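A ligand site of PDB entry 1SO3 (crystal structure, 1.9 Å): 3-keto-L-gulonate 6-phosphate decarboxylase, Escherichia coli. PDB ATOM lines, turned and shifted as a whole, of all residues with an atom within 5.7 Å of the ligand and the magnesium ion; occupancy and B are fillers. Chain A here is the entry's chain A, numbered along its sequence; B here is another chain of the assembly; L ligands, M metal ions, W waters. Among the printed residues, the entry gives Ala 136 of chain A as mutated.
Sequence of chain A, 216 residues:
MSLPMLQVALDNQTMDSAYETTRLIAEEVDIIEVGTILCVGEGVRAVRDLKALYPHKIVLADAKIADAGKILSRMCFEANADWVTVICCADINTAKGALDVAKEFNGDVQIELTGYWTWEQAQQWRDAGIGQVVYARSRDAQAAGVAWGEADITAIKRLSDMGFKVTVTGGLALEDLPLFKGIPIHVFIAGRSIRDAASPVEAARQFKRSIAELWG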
ATOM      1  N   ALA A   9      11.584   4.943   9.191  1.00  0.00           N
ATOM      2  CA  ALA A   9      12.747   5.639   8.663  1.00  0.00           C
ATOM      3  C   ALA A   9      12.402   7.116   8.531  1.00  0.00           C
ATOM      4  O   ALA A   9      11.497   7.487   7.760  1.00  0.00           O
ATOM      5  CB  ALA A   9      13.172   5.079   7.315  1.00  0.00           C
ATOM      6  N   ASP A  11      13.611   9.777   6.836  1.00  0.00           N
ATOM      7  CA  ASP A  11      14.383  10.329   5.735  1.00  0.00           C
ATOM      8  C   ASP A  11      13.878  11.731   5.442  1.00  0.00           C
ATOM      9  O   ASP A  11      13.241  11.990   4.444  1.00  0.00           O
ATOM     10  CB  ASP A  11      14.284   9.422   4.508  1.00  0.00           C
ATOM     11  CG  ASP A  11      15.053   8.132   4.701  1.00  0.00           C
ATOM     12  OD1 ASP A  11      16.203   8.256   5.175  1.00  0.00           O
ATOM     13  OD2 ASP A  11      14.587   6.977   4.473  1.00  0.00           O
ATOM     14  N   GLU A  33      14.493   5.428  13.244  1.00  0.00           N
ATOM     15  CA  GLU A  33      15.699   5.554  12.428  1.00  0.00           C
ATOM     16  C   GLU A  33      15.919   7.035  12.104  1.00  0.00           C
ATOM     17  O   GLU A  33      15.023   7.720  11.606  1.00  0.00           O
ATOM     18  CB  GLU A  33      15.583   4.748  11.124  1.00  0.00           C
ATOM     19  CG  GLU A  33      16.541   5.209  10.028  1.00  0.00           C
ATOM     20  CD  GLU A  33      16.401   4.488   8.699  1.00  0.00           C
ATOM     21  OE1 GLU A  33      15.866   3.364   8.671  1.00  0.00           O
ATOM     22  OE2 GLU A  33      16.847   5.034   7.660  1.00  0.00           O
ATOM     23  N   GLY A  35      17.324   8.652   9.417  1.00  0.00           N
ATOM     24  CA  GLY A  35      17.691   8.292   8.066  1.00  0.00           C
ATOM     25  C   GLY A  35      18.959   8.940   7.609  1.00  0.00           C
ATOM     26  O   GLY A  35      19.372   9.963   8.140  1.00  0.00           O
ATOM     27  N   THR A  36      19.592   8.351   6.595  1.00  0.00           N
ATOM     28  CA  THR A  36      20.799   8.947   6.031  1.00  0.00           C
ATOM     29  C   THR A  36      20.565  10.391   5.587  1.00  0.00           C
ATOM     30  O   THR A  36      21.403  11.253   5.777  1.00  0.00           O
ATOM     31  CB  THR A  36      21.336   8.121   4.870  1.00  0.00           C
ATOM     32  OG1 THR A  36      21.351   6.740   5.242  1.00  0.00           O
ATOM     33  CG2 THR A  36      22.834   8.500   4.628  1.00  0.00           C
ATOM     34  N   ASP A  62      21.332   5.735  10.652  1.00  0.00           N
ATOM     35  CA  ASP A  62      21.554   5.153   9.330  1.00  0.00           C
ATOM     36  C   ASP A  62      22.592   6.000   8.616  1.00  0.00           C
ATOM     37  O   ASP A  62      22.331   6.640   7.586  1.00  0.00           O
ATOM     38  CB  ASP A  62      20.236   5.042   8.524  1.00  0.00           C
ATOM     39  CG  ASP A  62      20.374   4.158   7.285  1.00  0.00           C
ATOM     40  OD1 ASP A  62      21.481   3.579   7.029  1.00  0.00           O
ATOM     41  OD2 ASP A  62      19.408   4.039   6.485  1.00  0.00           O
ATOM     42  N   LYS A  64      25.351   4.824   7.160  1.00  0.00           N
ATOM     43  CA  LYS A  64      25.966   4.129   6.022  1.00  0.00           C
ATOM     44  C   LYS A  64      27.475   4.378   5.982  1.00  0.00           C
ATOM     45  O   LYS A  64      28.045   4.733   4.953  1.00  0.00           O
ATOM     46  CB  LYS A  64      25.290   4.518   4.697  1.00  0.00           C
ATOM     47  CG  LYS A  64      23.826   3.971   4.589  1.00  0.00           C
ATOM     48  CD  LYS A  64      23.107   4.526   3.329  1.00  0.00           C
ATOM     49  CE  LYS A  64      21.796   3.805   3.069  1.00  0.00           C
ATOM     50  NZ  LYS A  64      20.745   4.163   4.092  1.00  0.00           N
ATOM     51  N   GLU A 112      24.701  -2.549   5.960  1.00  0.00           N
ATOM     52  CA  GLU A 112      23.637  -2.161   5.039  1.00  0.00           C
ATOM     53  C   GLU A 112      23.992  -2.744   3.695  1.00  0.00           C
ATOM     54  O   GLU A 112      25.031  -2.382   3.107  1.00  0.00           O
ATOM     55  CB  GLU A 112      23.525  -0.623   4.981  1.00  0.00           C
ATOM     56  CG  GLU A 112      22.330  -0.094   4.206  1.00  0.00           C
ATOM     57  CD  GLU A 112      21.070   0.105   5.056  1.00  0.00           C
ATOM     58  OE1 GLU A 112      20.093   0.620   4.494  1.00  0.00           O
ATOM     59  OE2 GLU A 112      21.062  -0.218   6.268  1.00  0.00           O
ATOM     60  N   THR A 114      23.098  -2.721   0.229  1.00  0.00           N
ATOM     61  CA  THR A 114      22.469  -1.953  -0.811  1.00  0.00           C
ATOM     62  C   THR A 114      23.488  -1.870  -1.941  1.00  0.00           C
ATOM     63  O   THR A 114      24.649  -1.557  -1.700  1.00  0.00           O
ATOM     64  CB  THR A 114      22.122  -0.562  -0.273  1.00  0.00           C
ATOM     65  OG1 THR A 114      21.157  -0.673   0.791  1.00  0.00           O
ATOM     66  CG2 THR A 114      21.438   0.257  -1.315  1.00  0.00           C
ATOM     67  N   ALA A 136      18.422  -4.307   1.846  1.00  0.00           N
ATOM     68  CA  ALA A 136      17.870  -2.971   1.547  1.00  0.00           C
ATOM     69  C   ALA A 136      17.840  -2.667   0.077  1.00  0.00           C
ATOM     70  O   ALA A 136      18.871  -2.199  -0.473  1.00  0.00           O
ATOM     71  CB  ALA A 136      18.705  -1.879   2.276  1.00  0.00           C
ATOM     72  N   ARG A 137      16.697  -2.864  -0.567  1.00  0.00           N
ATOM     73  CA  ARG A 137      16.548  -2.486  -1.953  1.00  0.00           C
ATOM     74  C   ARG A 137      16.751  -0.986  -2.162  1.00  0.00           C
ATOM     75  O   ARG A 137      16.042  -0.183  -1.584  1.00  0.00           O
ATOM     76  CB  ARG A 137      15.160  -2.872  -2.464  1.00  0.00           C
ATOM     77  CG  ARG A 137      14.850  -2.376  -3.851  1.00  0.00           C
ATOM     78  CD  ARG A 137      13.488  -2.807  -4.400  1.00  0.00           C
ATOM     79  NE  ARG A 137      12.371  -2.283  -3.601  1.00  0.00           N
ATOM     80  CZ  ARG A 137      11.118  -2.148  -4.046  1.00  0.00           C
ATOM     81  NH1 ARG A 137      10.766  -2.495  -5.293  1.00  0.00           N
ATOM     82  NH2 ARG A 137      10.186  -1.674  -3.238  1.00  0.00           N
ATOM     83  N   SER A 138      17.657  -0.636  -3.053  1.00  0.00           N
ATOM     84  CA  SER A 138      17.985   0.771  -3.291  1.00  0.00           C
ATOM     85  C   SER A 138      16.733   1.522  -3.741  1.00  0.00           C
ATOM     86  O   SER A 138      15.995   1.045  -4.615  1.00  0.00           O
ATOM     87  CB  SER A 138      19.099   0.878  -4.338  1.00  0.00           C
ATOM     88  OG  SER A 138      19.102   2.154  -4.954  1.00  0.00           O
ATOM     89  N   ARG A 139      16.521   2.696  -3.147  1.00  0.00           N
ATOM     90  CA  ARG A 139      15.491   3.631  -3.609  1.00  0.00           C
ATOM     91  C   ARG A 139      15.593   3.946  -5.135  1.00  0.00           C
ATOM     92  O   ARG A 139      14.576   4.097  -5.834  1.00  0.00           O
ATOM     93  CB  ARG A 139      15.627   4.919  -2.794  1.00  0.00           C
ATOM     94  CG  ARG A 139      14.841   6.084  -3.318  1.00  0.00           C
ATOM     95  CD  ARG A 139      15.124   7.410  -2.586  1.00  0.00           C
ATOM     96  NE  ARG A 139      14.994   7.295  -1.140  1.00  0.00           N
ATOM     97  CZ  ARG A 139      13.954   7.757  -0.413  1.00  0.00           C
ATOM     98  NH1 ARG A 139      12.938   8.416  -0.977  1.00  0.00           N
ATOM     99  NH2 ARG A 139      13.956   7.566   0.913  1.00  0.00           N
ATOM    100  N   GLN A 142      14.723   0.792  -7.152  1.00  0.00           N
ATOM    101  CA  GLN A 142      13.257   0.728  -7.080  1.00  0.00           C
ATOM    102  C   GLN A 142      12.619   1.710  -8.088  1.00  0.00           C
ATOM    103  O   GLN A 142      11.670   1.372  -8.808  1.00  0.00           O
ATOM    104  CB  GLN A 142      12.780   1.041  -5.665  1.00  0.00           C
ATOM    105  CG  GLN A 142      11.291   1.299  -5.532  1.00  0.00           C
ATOM    106  CD  GLN A 142      10.884   1.844  -4.178  1.00  0.00           C
ATOM    107  OE1 GLN A 142      11.733   2.077  -3.319  1.00  0.00           O
ATOM    108  NE2 GLN A 142       9.569   2.053  -3.999  1.00  0.00           N
ATOM    109  N   THR A 169      14.012  -4.016   4.003  1.00  0.00           N
ATOM    110  CA  THR A 169      13.602  -2.641   3.718  1.00  0.00           C
ATOM    111  C   THR A 169      13.793  -2.253   2.289  1.00  0.00           C
ATOM    112  O   THR A 169      14.529  -2.911   1.511  1.00  0.00           O
ATOM    113  CB  THR A 169      14.403  -1.685   4.655  1.00  0.00           C
ATOM    114  OG1 THR A 169      13.842  -0.366   4.581  1.00  0.00           O
ATOM    115  CG2 THR A 169      15.889  -1.531   4.194  1.00  0.00           C
ATOM    116  N   GLY A 170      13.110  -1.186   1.896  1.00  0.00           N
ATOM    117  CA  GLY A 170      13.351  -0.527   0.622  1.00  0.00           C
ATOM    118  C   GLY A 170      12.071  -0.400  -0.151  1.00  0.00           C
ATOM    119  O   GLY A 170      11.705  -1.299  -0.891  1.00  0.00           O
ATOM    120  N   GLY A 171      11.364   0.705   0.075  1.00  0.00           N
ATOM    121  CA  GLY A 171      10.059   0.951  -0.496  1.00  0.00           C
ATOM    122  C   GLY A 171       9.013  -0.092  -0.125  1.00  0.00           C
ATOM    123  O   GLY A 171       8.122  -0.359  -0.926  1.00  0.00           O
ATOM    124  N   LEU A 172       9.098  -0.683   1.060  1.00  0.00           N
ATOM    125  CA  LEU A 172       8.120  -1.678   1.479  1.00  0.00           C
ATOM    126  C   LEU A 172       6.725  -1.073   1.582  1.00  0.00           C
ATOM    127  O   LEU A 172       6.541   0.004   2.167  1.00  0.00           O
ATOM    128  CB  LEU A 172       8.482  -2.324   2.816  1.00  0.00           C
ATOM    129  CG  LEU A 172       9.528  -3.427   2.835  1.00  0.00           C
ATOM    130  CD1 LEU A 172       9.881  -3.815   4.261  1.00  0.00           C
ATOM    131  CD2 LEU A 172       9.117  -4.662   2.040  1.00  0.00           C
ATOM    132  N   ILE A 189      11.470  -2.253   8.001  1.00  0.00           N
ATOM    133  CA  ILE A 189      11.504  -0.795   7.997  1.00  0.00           C
ATOM    134  C   ILE A 189      10.499  -0.265   6.971  1.00  0.00           C
ATOM    135  O   ILE A 189      10.406  -0.811   5.867  1.00  0.00           O
ATOM    136  CB  ILE A 189      12.876  -0.270   7.582  1.00  0.00           C
ATOM    137  CG1 ILE A 189      13.997  -0.861   8.453  1.00  0.00           C
ATOM    138  CG2 ILE A 189      12.889   1.255   7.609  1.00  0.00           C
ATOM    139  CD1 ILE A 189      15.421  -0.456   8.026  1.00  0.00           C
ATOM    140  N   ALA A 190       9.813   0.812   7.343  1.00  0.00           N
ATOM    141  CA  ALA A 190       8.968   1.590   6.433  1.00  0.00           C
ATOM    142  C   ALA A 190       9.297   3.043   6.612  1.00  0.00           C
ATOM    143  O   ALA A 190       9.259   3.537   7.768  1.00  0.00           O
ATOM    144  CB  ALA A 190       7.509   1.412   6.756  1.00  0.00           C
ATOM    145  N   GLY A 191       9.587   3.735   5.514  1.00  0.00           N
ATOM    146  CA  GLY A 191       9.776   5.185   5.534  1.00  0.00           C
ATOM    147  C   GLY A 191       8.565   5.833   4.889  1.00  0.00           C
ATOM    148  O   GLY A 191       7.599   6.220   5.554  1.00  0.00           O
ATOM    149  N   ARG A 192       8.596   5.889   3.573  1.00  0.00           N
ATOM    150  CA  ARG A 192       7.565   6.558   2.786  1.00  0.00           C
ATOM    151  C   ARG A 192       6.147   6.008   3.066  1.00  0.00           C
ATOM    152  O   ARG A 192       5.210   6.771   3.204  1.00  0.00           O
ATOM    153  CB  ARG A 192       7.896   6.442   1.314  1.00  0.00           C
ATOM    154  CG  ARG A 192       8.997   7.411   0.856  1.00  0.00           C
ATOM    155  CD  ARG A 192       9.523   7.071  -0.529  1.00  0.00           C
ATOM    156  NE  ARG A 192      10.360   5.883  -0.451  1.00  0.00           N
ATOM    157  CZ  ARG A 192      10.772   5.200  -1.509  1.00  0.00           C
ATOM    158  NH1 ARG A 192      11.573   4.157  -1.342  1.00  0.00           N
ATOM    159  NH2 ARG A 192      10.453   5.593  -2.733  1.00  0.00           N
ATOM    160  N   SER A 193       6.028   4.687   3.141  1.00  0.00           N
ATOM    161  CA  SER A 193       4.716   4.015   3.328  1.00  0.00           C
ATOM    162  C   SER A 193       4.075   4.361   4.710  1.00  0.00           C
ATOM    163  O   SER A 193       2.851   4.220   4.883  1.00  0.00           O
ATOM    164  CB  SER A 193       4.900   2.486   3.095  1.00  0.00           C
ATOM    165  OG  SER A 193       5.314   1.864   4.269  1.00  0.00           O
ATOM    166  N   ARG A 195       5.341   7.652   6.589  1.00  0.00           N
ATOM    167  CA  ARG A 195       5.394   9.113   6.664  1.00  0.00           C
ATOM    168  C   ARG A 195       4.427   9.770   5.689  1.00  0.00           C
ATOM    169  O   ARG A 195       3.849  10.799   5.998  1.00  0.00           O
ATOM    170  CB  ARG A 195       6.784   9.644   6.291  1.00  0.00           C
ATOM    171  CG  ARG A 195       7.934   9.134   7.161  1.00  0.00           C
ATOM    172  CD  ARG A 195       9.188  10.051   7.095  1.00  0.00           C
ATOM    173  NE  ARG A 195       9.476  10.360   5.704  1.00  0.00           N
ATOM    174  CZ  ARG A 195      10.153   9.577   4.879  1.00  0.00           C
ATOM    175  NH1 ARG A 195      10.686   8.459   5.299  1.00  0.00           N
ATOM    176  NH2 ARG A 195      10.285   9.918   3.621  1.00  0.00           N
ATOM    177  N   ASP B  67      22.937   5.613  -1.529  1.00  0.00           N
ATOM    178  CA  ASP B  67      21.596   5.431  -2.068  1.00  0.00           C
ATOM    179  C   ASP B  67      20.970   6.799  -2.071  1.00  0.00           C
ATOM    180  O   ASP B  67      21.538   7.752  -1.489  1.00  0.00           O
ATOM    181  CB  ASP B  67      20.776   4.458  -1.189  1.00  0.00           C
ATOM    182  CG  ASP B  67      19.506   3.963  -1.876  1.00  0.00           C
ATOM    183  OD1 ASP B  67      19.398   4.074  -3.103  1.00  0.00           O
ATOM    184  OD2 ASP B  67      18.535   3.483  -1.244  1.00  0.00           O
ATOM    185  N   ALA B  68      19.832   6.919  -2.718  1.00  0.00           N
ATOM    186  CA  ALA B  68      19.074   8.161  -2.765  1.00  0.00           C
ATOM    187  C   ALA B  68      19.921   9.244  -3.405  1.00  0.00           C
ATOM    188  O   ALA B  68      20.052  10.384  -2.889  1.00  0.00           O
ATOM    189  CB  ALA B  68      18.625   8.560  -1.335  1.00  0.00           C
HETATM  190  O1  LIG L   1      12.315   3.069   1.282  1.00  0.00           O
HETATM  191  P1  LIG L   1      11.590   3.666   2.477  1.00  0.00           P
HETATM  192  O2  LIG L   1      10.980   5.049   2.122  1.00  0.00           O
HETATM  193  O3  LIG L   1      10.584   2.680   3.080  1.00  0.00           O
HETATM  194  O4  LIG L   1      12.712   3.983   3.586  1.00  0.00           O
HETATM  195  C1  LIG L   1      13.434   2.989   4.299  1.00  0.00           C
HETATM  196  C2  LIG L   1      14.781   2.736   3.612  1.00  0.00           C
HETATM  197  O5  LIG L   1      15.486   1.746   4.353  1.00  0.00           O
HETATM  198  C3  LIG L   1      15.573   4.052   3.592  1.00  0.00           C
HETATM  199  O6  LIG L   1      15.696   4.676   4.867  1.00  0.00           O
HETATM  200  C4  LIG L   1      16.965   3.783   3.103  1.00  0.00           C
HETATM  201  O7  LIG L   1      17.964   3.726   3.976  1.00  0.00           O
HETATM  202  N1  LIG L   1      17.104   3.607   1.871  1.00  0.00           N
HETATM  203  O8  LIG L   1      18.416   3.356   1.359  1.00  0.00           O
HETATM  204 MG    MG M   1      17.510   4.358   5.908  1.00  0.00          MG
HETATM  205  O   HOH W   1      20.268   1.182   2.127  1.00  0.00           O
HETATM  206  O   HOH W   2      10.851   0.076   3.231  1.00  0.00           O
HETATM  207  O   HOH W   3      16.679   6.305   0.832  1.00  0.00           O
HETATM  208  O   HOH W   4      17.988   6.277   5.227  1.00  0.00           O
HETATM  209  O   HOH W   5       8.041   2.502   2.319  1.00  0.00           O
HETATM  210  O   HOH W   6      12.241   7.214   3.286  1.00  0.00           O
HETATM  211  O   HOH W   7      16.966   2.364   6.420  1.00  0.00           O
HETATM  212  O   HOH W   8      14.832   3.228   0.127  1.00  0.00           O
HETATM  213  O   HOH W   9      19.108   6.509   2.395  1.00  0.00           O
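An oxygen (O6) of the ligand lies close to the side-chain carboxylate (OD2) of Asp 11, at 2.6 Å. The side-chain carboxylate (OD2) of Asp 67 of chain B lies within hydrogen-bond range of an oxygen (O8) of the ligand (2.6 Å). OG1 of Thr 169 sits at hydrogen-bond distance from O5 of the ligand, 2.7 Å away. The backbone NH (N) of Arg 192 sits at hydrogen-bond distance from an oxygen (O2) of the ligand. The guanidinium group (NE) of Arg 192 is in salt-bridge range of an oxygen (O2) of the ligand, 2.8 Å away. An oxygen (O7) of the ligand lies close to the side-chain amino group (NZ) of Lys 64 (2.8 Å). N of Gly 171 sits at hydrogen-bond distance from O1 of the ligand, 2.8 Å away. N of Gly 191 is in hydrogen-bond range of O3 of the ligand (2.8 Å).
The side-chain carboxylate (OD1) of Asp 62 lies within salt-bridge range of the side-chain amino group (NZ) of Lys 64 (3.1 Å). The side-chain hydroxyl (OG1) of Thr 36 is in hydrogen-bond range of the backbone carbonyl oxygen (O) of Asp 62 (2.5 Å). OD2 of Asp 67 of chain B sits at hydrogen-bond distance from N of Arg 139, at 2.9 Å. OD1 of Asp 67 of chain B lies within hydrogen-bond range of OG of Ser 138. The backbone NH (N) of Arg 137 is in hydrogen-bond range of the backbone carbonyl oxygen (O) of Thr 169 (3.0 Å). NH1 of Arg 192 is in hydrogen-bond range of OE1 of Gln 142, 2.9 Å away. The side-chain hydroxyl (OG1) of Thr 36 lies within hydrogen-bond range of the side-chain amino group (NZ) of Lys 64, at 2.9 Å. O of Ala 9 lies within hydrogen-bond range of NH1 of Arg 195, at 2.8 Å.
Ala 9 touches the ligand. Glu 112 touches the ligand (OE1 to O7, 3.8 Å). C of Gly 170 touches O1 of the ligand (3.8 Å). CG2 of Ile 189 touches C1 of the ligand, 3.8 Å away. C of Ala 190 touches O3 of the ligand (3.8 Å). Hydrophobic or aromatic side chains that line the ligand: Ala 9 and Ile 189. 14 residues have an atom within 4 Å of the ligand: Ala 9, Asp 11, Glu 33, Asp 62, Lys 64, Glu 112, Thr 169, Gly 170, Gly 171, Ile 189, Ala 190, Gly 191, Arg 192 and Asp 67 of chain B.
Merely in contact with the magnesium ion: Lys 64. Of the 26 residues printed, 3 come within 4 Å of the magnesium ion. Along chain A the residues within 4 Å of the magnesium ion span positions 33 to 64. The nearest printed residue that does not touch the magnesium ion is Asp 11 (4.2 Å).
The magnesium ion is bound by OE2 of Glu 33 (2.0 Å), OD2 of Asp 62 (2.0 Å), O7 of the ligand (2.1 Å), water W4 (2.1 Å), O6 of the ligand (2.1 Å) and water W7 (2.1 Å).
Water W4 lies within hydrogen-bond range of the side-chain carboxylate of Asp 11 (2.7 Å) and the backbone NH of Thr 36 (3.0 Å). Water W7 bridges an oxygen (O5) of the ligand and the side-chain carboxylate (OE1) of Glu 33. Water W5 lies within hydrogen-bond range of O3 of the ligand, O of Leu 172 and N of Ser 193. Water W3 bridges NE of Arg 139 and N1 of the ligand. Water W1 lies within hydrogen-bond range of the side-chain carboxylate of Glu 112 (2.4 Å), the side-chain hydroxyl of Thr 114 (2.5 Å) and an oxygen (O8) of the ligand (3.0 Å). Water W9 bridges NZ of Lys 64 (3.3 Å) and O8 of the ligand (3.4 Å).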
